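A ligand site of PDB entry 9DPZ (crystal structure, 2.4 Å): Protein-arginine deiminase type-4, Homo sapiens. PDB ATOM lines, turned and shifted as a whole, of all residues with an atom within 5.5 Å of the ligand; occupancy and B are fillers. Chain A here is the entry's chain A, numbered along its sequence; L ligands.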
ATOM      1  N   ASP A 358     -19.830  16.666  28.907  1.00  0.00           N
ATOM      2  CA  ASP A 358     -18.665  15.762  28.960  1.00  0.00           C
ATOM      3  C   ASP A 358     -17.560  16.243  29.978  1.00  0.00           C
ATOM      4  O   ASP A 358     -16.433  15.707  29.945  1.00  0.00           O
ATOM      5  CB  ASP A 358     -18.023  15.596  27.576  1.00  0.00           C
ATOM      6  CG  ASP A 358     -18.957  14.962  26.540  1.00  0.00           C
ATOM      7  OD1 ASP A 358     -20.202  14.930  26.740  1.00  0.00           O
ATOM      8  OD2 ASP A 358     -18.429  14.486  25.510  1.00  0.00           O
ATOM      9  N   GLY A 416     -16.025  12.065  27.941  1.00  0.00           N
ATOM     10  CA  GLY A 416     -16.474  11.830  26.593  1.00  0.00           C
ATOM     11  C   GLY A 416     -15.780  10.673  25.929  1.00  0.00           C
ATOM     12  O   GLY A 416     -16.296  10.136  24.949  1.00  0.00           O
ATOM     13  N   ASN A 417     -14.631  10.262  26.470  1.00  0.00           N
ATOM     14  CA  ASN A 417     -13.881   9.114  25.975  1.00  0.00           C
ATOM     15  C   ASN A 417     -14.103   7.864  26.829  1.00  0.00           C
ATOM     16  O   ASN A 417     -13.198   7.039  26.955  1.00  0.00           O
ATOM     17  CB  ASN A 417     -12.405   9.463  25.922  1.00  0.00           C
ATOM     18  CG  ASN A 417     -11.632   8.475  25.105  1.00  0.00           C
ATOM     19  OD1 ASN A 417     -12.200   7.703  24.338  1.00  0.00           O
ATOM     20  ND2 ASN A 417     -10.310   8.482  25.276  1.00  0.00           N
ATOM     21  N   SER A 476     -10.352  13.582  15.539  1.00  0.00           N
ATOM     22  CA  SER A 476      -9.735  14.868  15.845  1.00  0.00           C
ATOM     23  C   SER A 476      -9.745  15.140  17.342  1.00  0.00           C
ATOM     24  O   SER A 476      -8.696  15.476  17.911  1.00  0.00           O
ATOM     25  CB  SER A 476     -10.441  16.011  15.125  1.00  0.00           C
ATOM     26  OG  SER A 476      -9.840  17.238  15.527  1.00  0.00           O
ATOM     27  N   VAL A 477     -10.902  14.988  17.990  1.00  0.00           N
ATOM     28  CA  VAL A 477     -11.021  15.129  19.435  1.00  0.00           C
ATOM     29  C   VAL A 477     -10.613  13.853  20.183  1.00  0.00           C
ATOM     30  O   VAL A 477     -10.016  13.932  21.259  1.00  0.00           O
ATOM     31  CB  VAL A 477     -12.450  15.578  19.800  1.00  0.00           C
ATOM     32  CG1 VAL A 477     -12.616  17.053  19.486  1.00  0.00           C
ATOM     33  CG2 VAL A 477     -13.445  14.787  19.021  1.00  0.00           C
ATOM     34  N   HIS A 479     -12.585  10.756  21.016  1.00  0.00           N
ATOM     35  CA  HIS A 479     -13.467  10.124  21.974  1.00  0.00           C
ATOM     36  C   HIS A 479     -14.244   8.954  21.362  1.00  0.00           C
ATOM     37  O   HIS A 479     -14.858   9.107  20.307  1.00  0.00           O
ATOM     38  CB  HIS A 479     -14.450  11.159  22.516  1.00  0.00           C
ATOM     39  CG  HIS A 479     -13.781  12.270  23.232  1.00  0.00           C
ATOM     40  ND1 HIS A 479     -14.475  13.270  23.878  1.00  0.00           N
ATOM     41  CD2 HIS A 479     -12.464  12.549  23.408  1.00  0.00           C
ATOM     42  CE1 HIS A 479     -13.630  14.120  24.410  1.00  0.00           C
ATOM     43  NE2 HIS A 479     -12.398  13.703  24.154  1.00  0.00           N
ATOM     44  N   ASP A 481     -17.035   7.949  22.148  1.00  0.00           N
ATOM     45  CA  ASP A 481     -18.492   8.129  22.031  1.00  0.00           C
ATOM     46  C   ASP A 481     -18.895   8.747  20.714  1.00  0.00           C
ATOM     47  O   ASP A 481     -20.092   8.946  20.468  1.00  0.00           O
ATOM     48  CB  ASP A 481     -19.055   8.956  23.218  1.00  0.00           C
ATOM     49  CG  ASP A 481     -18.860  10.477  23.061  1.00  0.00           C
ATOM     50  OD1 ASP A 481     -17.861  10.918  22.450  1.00  0.00           O
ATOM     51  OD2 ASP A 481     -19.709  11.243  23.584  1.00  0.00           O
ATOM     52  N   GLU A 482     -17.933   9.025  19.837  1.00  0.00           N
ATOM     53  CA  GLU A 482     -18.196   9.613  18.546  1.00  0.00           C
ATOM     54  C   GLU A 482     -18.537   8.591  17.470  1.00  0.00           C
ATOM     55  O   GLU A 482     -19.118   8.962  16.441  1.00  0.00           O
ATOM     56  CB  GLU A 482     -16.988  10.395  18.079  1.00  0.00           C
ATOM     57  CG  GLU A 482     -16.727  11.626  18.864  1.00  0.00           C
ATOM     58  CD  GLU A 482     -15.413  12.225  18.431  1.00  0.00           C
ATOM     59  OE1 GLU A 482     -15.407  13.066  17.488  1.00  0.00           O
ATOM     60  OE2 GLU A 482     -14.384  11.827  18.999  1.00  0.00           O
ATOM     61  N   PHE A 523     -27.048  19.598   4.034  1.00  0.00           N
ATOM     62  CA  PHE A 523     -26.860  20.835   4.800  1.00  0.00           C
ATOM     63  C   PHE A 523     -27.997  21.825   4.564  1.00  0.00           C
ATOM     64  O   PHE A 523     -27.806  23.028   4.733  1.00  0.00           O
ATOM     65  CB  PHE A 523     -25.512  21.503   4.496  1.00  0.00           C
ATOM     66  CG  PHE A 523     -24.330  20.602   4.743  1.00  0.00           C
ATOM     67  CD1 PHE A 523     -23.650  20.646   5.948  1.00  0.00           C
ATOM     68  CD2 PHE A 523     -23.918  19.716   3.766  1.00  0.00           C
ATOM     69  CE1 PHE A 523     -22.569  19.809   6.175  1.00  0.00           C
ATOM     70  CE2 PHE A 523     -22.849  18.875   3.982  1.00  0.00           C
ATOM     71  CZ  PHE A 523     -22.165  18.929   5.188  1.00  0.00           C
ATOM     72  N   ILE A 526     -29.249  25.662   6.747  1.00  0.00           N
ATOM     73  CA  ILE A 526     -28.021  26.136   7.387  1.00  0.00           C
ATOM     74  C   ILE A 526     -27.207  26.932   6.379  1.00  0.00           C
ATOM     75  O   ILE A 526     -27.125  26.553   5.208  1.00  0.00           O
ATOM     76  CB  ILE A 526     -27.148  24.975   7.914  1.00  0.00           C
ATOM     77  CG1 ILE A 526     -27.797  24.214   9.055  1.00  0.00           C
ATOM     78  CG2 ILE A 526     -25.802  25.497   8.399  1.00  0.00           C
ATOM     79  CD1 ILE A 526     -26.790  23.420   9.831  1.00  0.00           C
ATOM     80  N   LYS A 580     -14.967  13.590   7.734  1.00  0.00           N
ATOM     81  CA  LYS A 580     -14.013  14.398   6.986  1.00  0.00           C
ATOM     82  C   LYS A 580     -12.766  14.556   7.832  1.00  0.00           C
ATOM     83  O   LYS A 580     -12.838  14.574   9.065  1.00  0.00           O
ATOM     84  CB  LYS A 580     -14.608  15.772   6.604  1.00  0.00           C
ATOM     85  CG  LYS A 580     -14.909  16.728   7.759  1.00  0.00           C
ATOM     86  CD  LYS A 580     -15.538  18.063   7.281  1.00  0.00           C
ATOM     87  CE  LYS A 580     -15.780  19.008   8.462  1.00  0.00           C
ATOM     88  NZ  LYS A 580     -17.210  19.415   8.603  1.00  0.00           N
ATOM     89  N   GLU A 588     -13.515  13.699  11.791  1.00  0.00           N
ATOM     90  CA  GLU A 588     -14.513  14.618  12.334  1.00  0.00           C
ATOM     91  C   GLU A 588     -15.827  14.355  11.625  1.00  0.00           C
ATOM     92  O   GLU A 588     -15.849  13.972  10.452  1.00  0.00           O
ATOM     93  CB  GLU A 588     -14.083  16.081  12.133  1.00  0.00           C
ATOM     94  CG  GLU A 588     -14.948  17.130  12.820  1.00  0.00           C
ATOM     95  CD  GLU A 588     -14.343  18.537  12.728  1.00  0.00           C
ATOM     96  OE1 GLU A 588     -13.113  18.624  12.509  1.00  0.00           O
ATOM     97  OE2 GLU A 588     -15.092  19.535  12.862  1.00  0.00           O
ATOM     98  N   ALA A 589     -16.921  14.557  12.350  1.00  0.00           N
ATOM     99  CA  ALA A 589     -18.236  14.337  11.754  1.00  0.00           C
ATOM    100  C   ALA A 589     -18.433  15.264  10.560  1.00  0.00           C
ATOM    101  O   ALA A 589     -18.153  16.467  10.629  1.00  0.00           O
ATOM    102  CB  ALA A 589     -19.343  14.567  12.782  1.00  0.00           C
ATOM    103  N   PHE A 590     -18.902  14.684   9.452  1.00  0.00           N
ATOM    104  CA  PHE A 590     -19.228  15.503   8.297  1.00  0.00           C
ATOM    105  C   PHE A 590     -20.532  16.232   8.520  1.00  0.00           C
ATOM    106  O   PHE A 590     -20.604  17.452   8.335  1.00  0.00           O
ATOM    107  CB  PHE A 590     -19.295  14.646   7.032  1.00  0.00           C
ATOM    108  CG  PHE A 590     -19.408  15.461   5.761  1.00  0.00           C
ATOM    109  CD1 PHE A 590     -19.016  16.798   5.739  1.00  0.00           C
ATOM    110  CD2 PHE A 590     -19.916  14.906   4.599  1.00  0.00           C
ATOM    111  CE1 PHE A 590     -19.132  17.543   4.595  1.00  0.00           C
ATOM    112  CE2 PHE A 590     -20.031  15.652   3.445  1.00  0.00           C
ATOM    113  CZ  PHE A 590     -19.636  16.974   3.444  1.00  0.00           C
ATOM    114  N   PHE A 591     -21.574  15.513   8.889  1.00  0.00           N
ATOM    115  CA  PHE A 591     -22.831  16.075   9.362  1.00  0.00           C
ATOM    116  C   PHE A 591     -23.066  15.622  10.802  1.00  0.00           C
ATOM    117  O   PHE A 591     -22.371  14.716  11.281  1.00  0.00           O
ATOM    118  CB  PHE A 591     -23.990  15.657   8.431  1.00  0.00           C
ATOM    119  CG  PHE A 591     -24.131  14.181   8.254  1.00  0.00           C
ATOM    120  CD1 PHE A 591     -24.541  13.387   9.311  1.00  0.00           C
ATOM    121  CD2 PHE A 591     -23.884  13.588   7.031  1.00  0.00           C
ATOM    122  CE1 PHE A 591     -24.683  12.022   9.159  1.00  0.00           C
ATOM    123  CE2 PHE A 591     -24.023  12.223   6.859  1.00  0.00           C
ATOM    124  CZ  PHE A 591     -24.431  11.437   7.937  1.00  0.00           C
ATOM    125  N   PRO A 592     -23.992  16.256  11.540  1.00  0.00           N
ATOM    126  CA  PRO A 592     -24.138  15.950  12.969  1.00  0.00           C
ATOM    127  C   PRO A 592     -24.097  14.458  13.297  1.00  0.00           C
ATOM    128  O   PRO A 592     -24.701  13.628  12.603  1.00  0.00           O
ATOM    129  CB  PRO A 592     -25.498  16.571  13.301  1.00  0.00           C
ATOM    130  CG  PRO A 592     -25.557  17.753  12.409  1.00  0.00           C
ATOM    131  CD  PRO A 592     -24.890  17.348  11.127  1.00  0.00           C
ATOM    132  N   ASN A 593     -23.364  14.121  14.346  1.00  0.00           N
ATOM    133  CA  ASN A 593     -22.935  12.748  14.577  1.00  0.00           C
ATOM    134  C   ASN A 593     -24.068  11.943  15.202  1.00  0.00           C
ATOM    135  O   ASN A 593     -24.203  11.904  16.424  1.00  0.00           O
ATOM    136  CB  ASN A 593     -21.706  12.728  15.472  1.00  0.00           C
ATOM    137  CG  ASN A 593     -20.927  11.458  15.316  1.00  0.00           C
ATOM    138  OD1 ASN A 593     -21.497  10.377  15.279  1.00  0.00           O
ATOM    139  ND2 ASN A 593     -19.605  11.580  15.171  1.00  0.00           N
ATOM    140  N   ASN A 596     -24.109   9.365  18.347  1.00  0.00           N
ATOM    141  CA  ASN A 596     -23.932   9.885  19.698  1.00  0.00           C
ATOM    142  C   ASN A 596     -25.265  10.437  20.211  1.00  0.00           C
ATOM    143  O   ASN A 596     -25.386  11.611  20.542  1.00  0.00           O
ATOM    144  CB  ASN A 596     -22.834  10.951  19.697  1.00  0.00           C
ATOM    145  CG  ASN A 596     -22.451  11.417  21.091  1.00  0.00           C
ATOM    146  OD1 ASN A 596     -22.817  10.809  22.103  1.00  0.00           O
ATOM    147  ND2 ASN A 596     -21.697  12.505  21.141  1.00  0.00           N
ATOM    148  N   PHE A 610     -29.843  16.805   9.061  1.00  0.00           N
ATOM    149  CA  PHE A 610     -30.026  17.780   7.982  1.00  0.00           C
ATOM    150  C   PHE A 610     -29.576  17.187   6.643  1.00  0.00           C
ATOM    151  O   PHE A 610     -28.876  17.824   5.855  1.00  0.00           O
ATOM    152  CB  PHE A 610     -29.314  19.112   8.252  1.00  0.00           C
ATOM    153  CG  PHE A 610     -29.842  19.875   9.439  1.00  0.00           C
ATOM    154  CD1 PHE A 610     -31.191  19.740   9.812  1.00  0.00           C
ATOM    155  CD2 PHE A 610     -29.007  20.704  10.201  1.00  0.00           C
ATOM    156  CE1 PHE A 610     -31.698  20.423  10.917  1.00  0.00           C
ATOM    157  CE2 PHE A 610     -29.504  21.382  11.297  1.00  0.00           C
ATOM    158  CZ  PHE A 610     -30.866  21.243  11.668  1.00  0.00           C
ATOM    159  N   PHE A 642     -26.003  19.644  18.974  1.00  0.00           N
ATOM    160  CA  PHE A 642     -24.646  20.061  19.243  1.00  0.00           C
ATOM    161  C   PHE A 642     -24.489  21.550  18.949  1.00  0.00           C
ATOM    162  O   PHE A 642     -25.161  22.097  18.059  1.00  0.00           O
ATOM    163  CB  PHE A 642     -23.652  19.279  18.413  1.00  0.00           C
ATOM    164  CG  PHE A 642     -23.674  17.805  18.674  1.00  0.00           C
ATOM    165  CD1 PHE A 642     -24.406  16.950  17.873  1.00  0.00           C
ATOM    166  CD2 PHE A 642     -22.919  17.267  19.695  1.00  0.00           C
ATOM    167  CE1 PHE A 642     -24.389  15.586  18.084  1.00  0.00           C
ATOM    168  CE2 PHE A 642     -22.913  15.906  19.925  1.00  0.00           C
ATOM    169  CZ  PHE A 642     -23.656  15.070  19.114  1.00  0.00           C
ATOM    170  N   THR A 643     -23.573  22.182  19.690  1.00  0.00           N
ATOM    171  CA  THR A 643     -23.331  23.620  19.656  1.00  0.00           C
ATOM    172  C   THR A 643     -21.843  23.863  19.487  1.00  0.00           C
ATOM    173  O   THR A 643     -21.016  23.198  20.127  1.00  0.00           O
ATOM    174  CB  THR A 643     -23.842  24.283  20.941  1.00  0.00           C
ATOM    175  OG1 THR A 643     -22.877  24.132  21.998  1.00  0.00           O
ATOM    176  CG2 THR A 643     -25.162  23.652  21.381  1.00  0.00           C
ATOM    177  N   TYR A 644     -21.494  24.812  18.622  1.00  0.00           N
ATOM    178  CA  TYR A 644     -20.104  25.145  18.305  1.00  0.00           C
ATOM    179  C   TYR A 644     -19.694  26.379  19.098  1.00  0.00           C
ATOM    180  O   TYR A 644     -20.373  27.409  19.030  1.00  0.00           O
ATOM    181  CB  TYR A 644     -19.950  25.387  16.804  1.00  0.00           C
ATOM    182  CG  TYR A 644     -18.566  25.142  16.243  1.00  0.00           C
ATOM    183  CD1 TYR A 644     -17.563  26.109  16.346  1.00  0.00           C
ATOM    184  CD2 TYR A 644     -18.261  23.957  15.590  1.00  0.00           C
ATOM    185  CE1 TYR A 644     -16.287  25.881  15.824  1.00  0.00           C
ATOM    186  CE2 TYR A 644     -16.990  23.720  15.067  1.00  0.00           C
ATOM    187  CZ  TYR A 644     -16.012  24.686  15.187  1.00  0.00           C
ATOM    188  OH  TYR A 644     -14.754  24.445  14.662  1.00  0.00           O
ATOM    189  N   VAL A 651     -16.987  21.576  19.915  1.00  0.00           N
ATOM    190  CA  VAL A 651     -18.313  21.004  19.783  1.00  0.00           C
ATOM    191  C   VAL A 651     -18.770  20.458  21.140  1.00  0.00           C
ATOM    192  O   VAL A 651     -18.054  19.690  21.791  1.00  0.00           O
ATOM    193  CB  VAL A 651     -18.312  19.899  18.704  1.00  0.00           C
ATOM    194  CG1 VAL A 651     -19.688  19.310  18.535  1.00  0.00           C
ATOM    195  CG2 VAL A 651     -17.787  20.451  17.375  1.00  0.00           C
ATOM    196  N   HIS A 652     -19.981  20.857  21.559  1.00  0.00           N
ATOM    197  CA  HIS A 652     -20.521  20.538  22.888  1.00  0.00           C
ATOM    198  C   HIS A 652     -21.974  20.050  22.776  1.00  0.00           C
ATOM    199  O   HIS A 652     -22.641  20.237  21.756  1.00  0.00           O
ATOM    200  CB  HIS A 652     -20.458  21.762  23.830  1.00  0.00           C
ATOM    201  CG  HIS A 652     -19.097  22.027  24.413  1.00  0.00           C
ATOM    202  ND1 HIS A 652     -18.728  23.260  24.908  1.00  0.00           N
ATOM    203  CD2 HIS A 652     -18.025  21.210  24.611  1.00  0.00           C
ATOM    204  CE1 HIS A 652     -17.487  23.206  25.369  1.00  0.00           C
ATOM    205  NE2 HIS A 652     -17.039  21.971  25.196  1.00  0.00           N
HETATM  206  C1  LIG L   1     -23.206  20.515   9.405  1.00  0.00           C
HETATM  207  C2  LIG L   1     -22.338  19.461   9.625  1.00  0.00           C
HETATM  208  C3  LIG L   1     -21.202  18.132  11.608  1.00  0.00           C
HETATM  209  C4  LIG L   1     -20.493  15.600  16.905  1.00  0.00           C
HETATM  210  C5  LIG L   1     -18.134  15.846  17.357  1.00  0.00           C
HETATM  211  C6  LIG L   1     -23.751  21.185  10.494  1.00  0.00           C
HETATM  212  C7  LIG L   1     -22.048  19.081  10.941  1.00  0.00           C
HETATM  213  C8  LIG L   1     -19.381  15.314  17.691  1.00  0.00           C
HETATM  214  C9  LIG L   1     -20.345  16.421  15.787  1.00  0.00           C
HETATM  215  C10 LIG L   1     -19.095  16.962  15.464  1.00  0.00           C
HETATM  216  C11 LIG L   1     -17.988  16.667  16.259  1.00  0.00           C
HETATM  217  C12 LIG L   1     -21.340  18.328  12.964  1.00  0.00           C
HETATM  218  C13 LIG L   1     -22.623  19.877  11.953  1.00  0.00           C
HETATM  219  C14 LIG L   1     -20.665  17.622  14.037  1.00  0.00           C
HETATM  220  C15 LIG L   1     -19.592  14.478  18.921  1.00  0.00           C
HETATM  221  C16 LIG L   1     -20.739  21.444  14.678  1.00  0.00           C
HETATM  222  C17 LIG L   1     -21.130  21.364  16.110  1.00  0.00           C
HETATM  223  C18 LIG L   1     -17.450  16.579  20.768  1.00  0.00           C
HETATM  224  C19 LIG L   1     -18.892  16.405  20.341  1.00  0.00           C
HETATM  225  C20 LIG L   1     -18.995  14.188  21.329  1.00  0.00           C
HETATM  226  C21 LIG L   1     -22.149  21.149  15.046  1.00  0.00           C
HETATM  227  C22 LIG L   1     -17.559  14.293  21.792  1.00  0.00           C
HETATM  228  C23 LIG L   1     -17.139  15.747  22.002  1.00  0.00           C
HETATM  229  C24 LIG L   1     -18.344  18.546  13.583  1.00  0.00           C
HETATM  230  C25 LIG L   1     -15.630  16.870  16.597  1.00  0.00           C
HETATM  231  C26 LIG L   1     -22.684  19.871  14.508  1.00  0.00           C
HETATM  232  N1  LIG L   1     -23.486  20.880  11.771  1.00  0.00           N
HETATM  233  N2  LIG L   1     -21.316  16.851  14.885  1.00  0.00           N
HETATM  234  N3  LIG L   1     -19.328  17.743  14.317  1.00  0.00           N
HETATM  235  N4  LIG L   1     -22.219  19.379  13.206  1.00  0.00           N
HETATM  236  N5  LIG L   1     -19.202  14.986  20.116  1.00  0.00           N
HETATM  237  N6  LIG L   1     -17.364  13.527  23.065  1.00  0.00           N
HETATM  238  O1  LIG L   1     -20.146  13.395  18.825  1.00  0.00           O
HETATM  239  O2  LIG L   1     -17.834  16.287  23.127  1.00  0.00           O
HETATM  240  O3  LIG L   1     -16.794  17.190  15.837  1.00  0.00           O
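OD2 of Asp 481 sits at hydrogen-bond distance from ND2 of Asn 596, 3.4 Å away. The side-chain carboxylate (OE2) of Glu 482 sits at hydrogen-bond distance from the backbone NH (N) of His 479. The backbone carbonyl oxygen (O) of Phe 610 lies within hydrogen-bond range of the backbone NH (N) of Phe 523 (3.1 Å). The backbone carbonyl oxygen of Glu 482 is in hydrogen-bond range of the side-chain amide nitrogen of Asn 593 (3.0 Å). The backbone carbonyl oxygen (O) of Glu 588 lies within hydrogen-bond range of the backbone NH (N) of Lys 580 (2.9 Å).
The side-chain carboxylate (OD1) of Asp 481 lies within salt-bridge range of a nitrogen (N6) of the ligand (2.7 Å). The side-chain carboxylate (OD2) of Asp 358 lies within salt-bridge range of a nitrogen (N6) of the ligand, 2.8 Å away. The side-chain amide nitrogen of Asn 596 sits at hydrogen-bond distance from an oxygen (O1) of the ligand (2.9 Å). ND1 of His 479 lies within hydrogen-bond range of N6 of the ligand (3.0 Å). A nitrogen (N2) of the ligand is in hydrogen-bond range of the backbone NH of Asn 593 (3.5 Å).
Residues that only touch the ligand: Val 477 (3.9 Å), Glu 482 (3.8 Å), Phe 523 (3.4 Å), Ile 526 (3.8 Å), Glu 588 (3.5 Å), Ala 589 (3.5 Å), Phe 590 (3.0 Å), Phe 591 (3.2 Å), Pro 592 (3.3 Å), Phe 642 (3.8 Å), Tyr 644 (3.6 Å) and Val 651 (3.3 Å). The nearest printed residue that does not touch the ligand is Gly 416 (4.01 Å).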
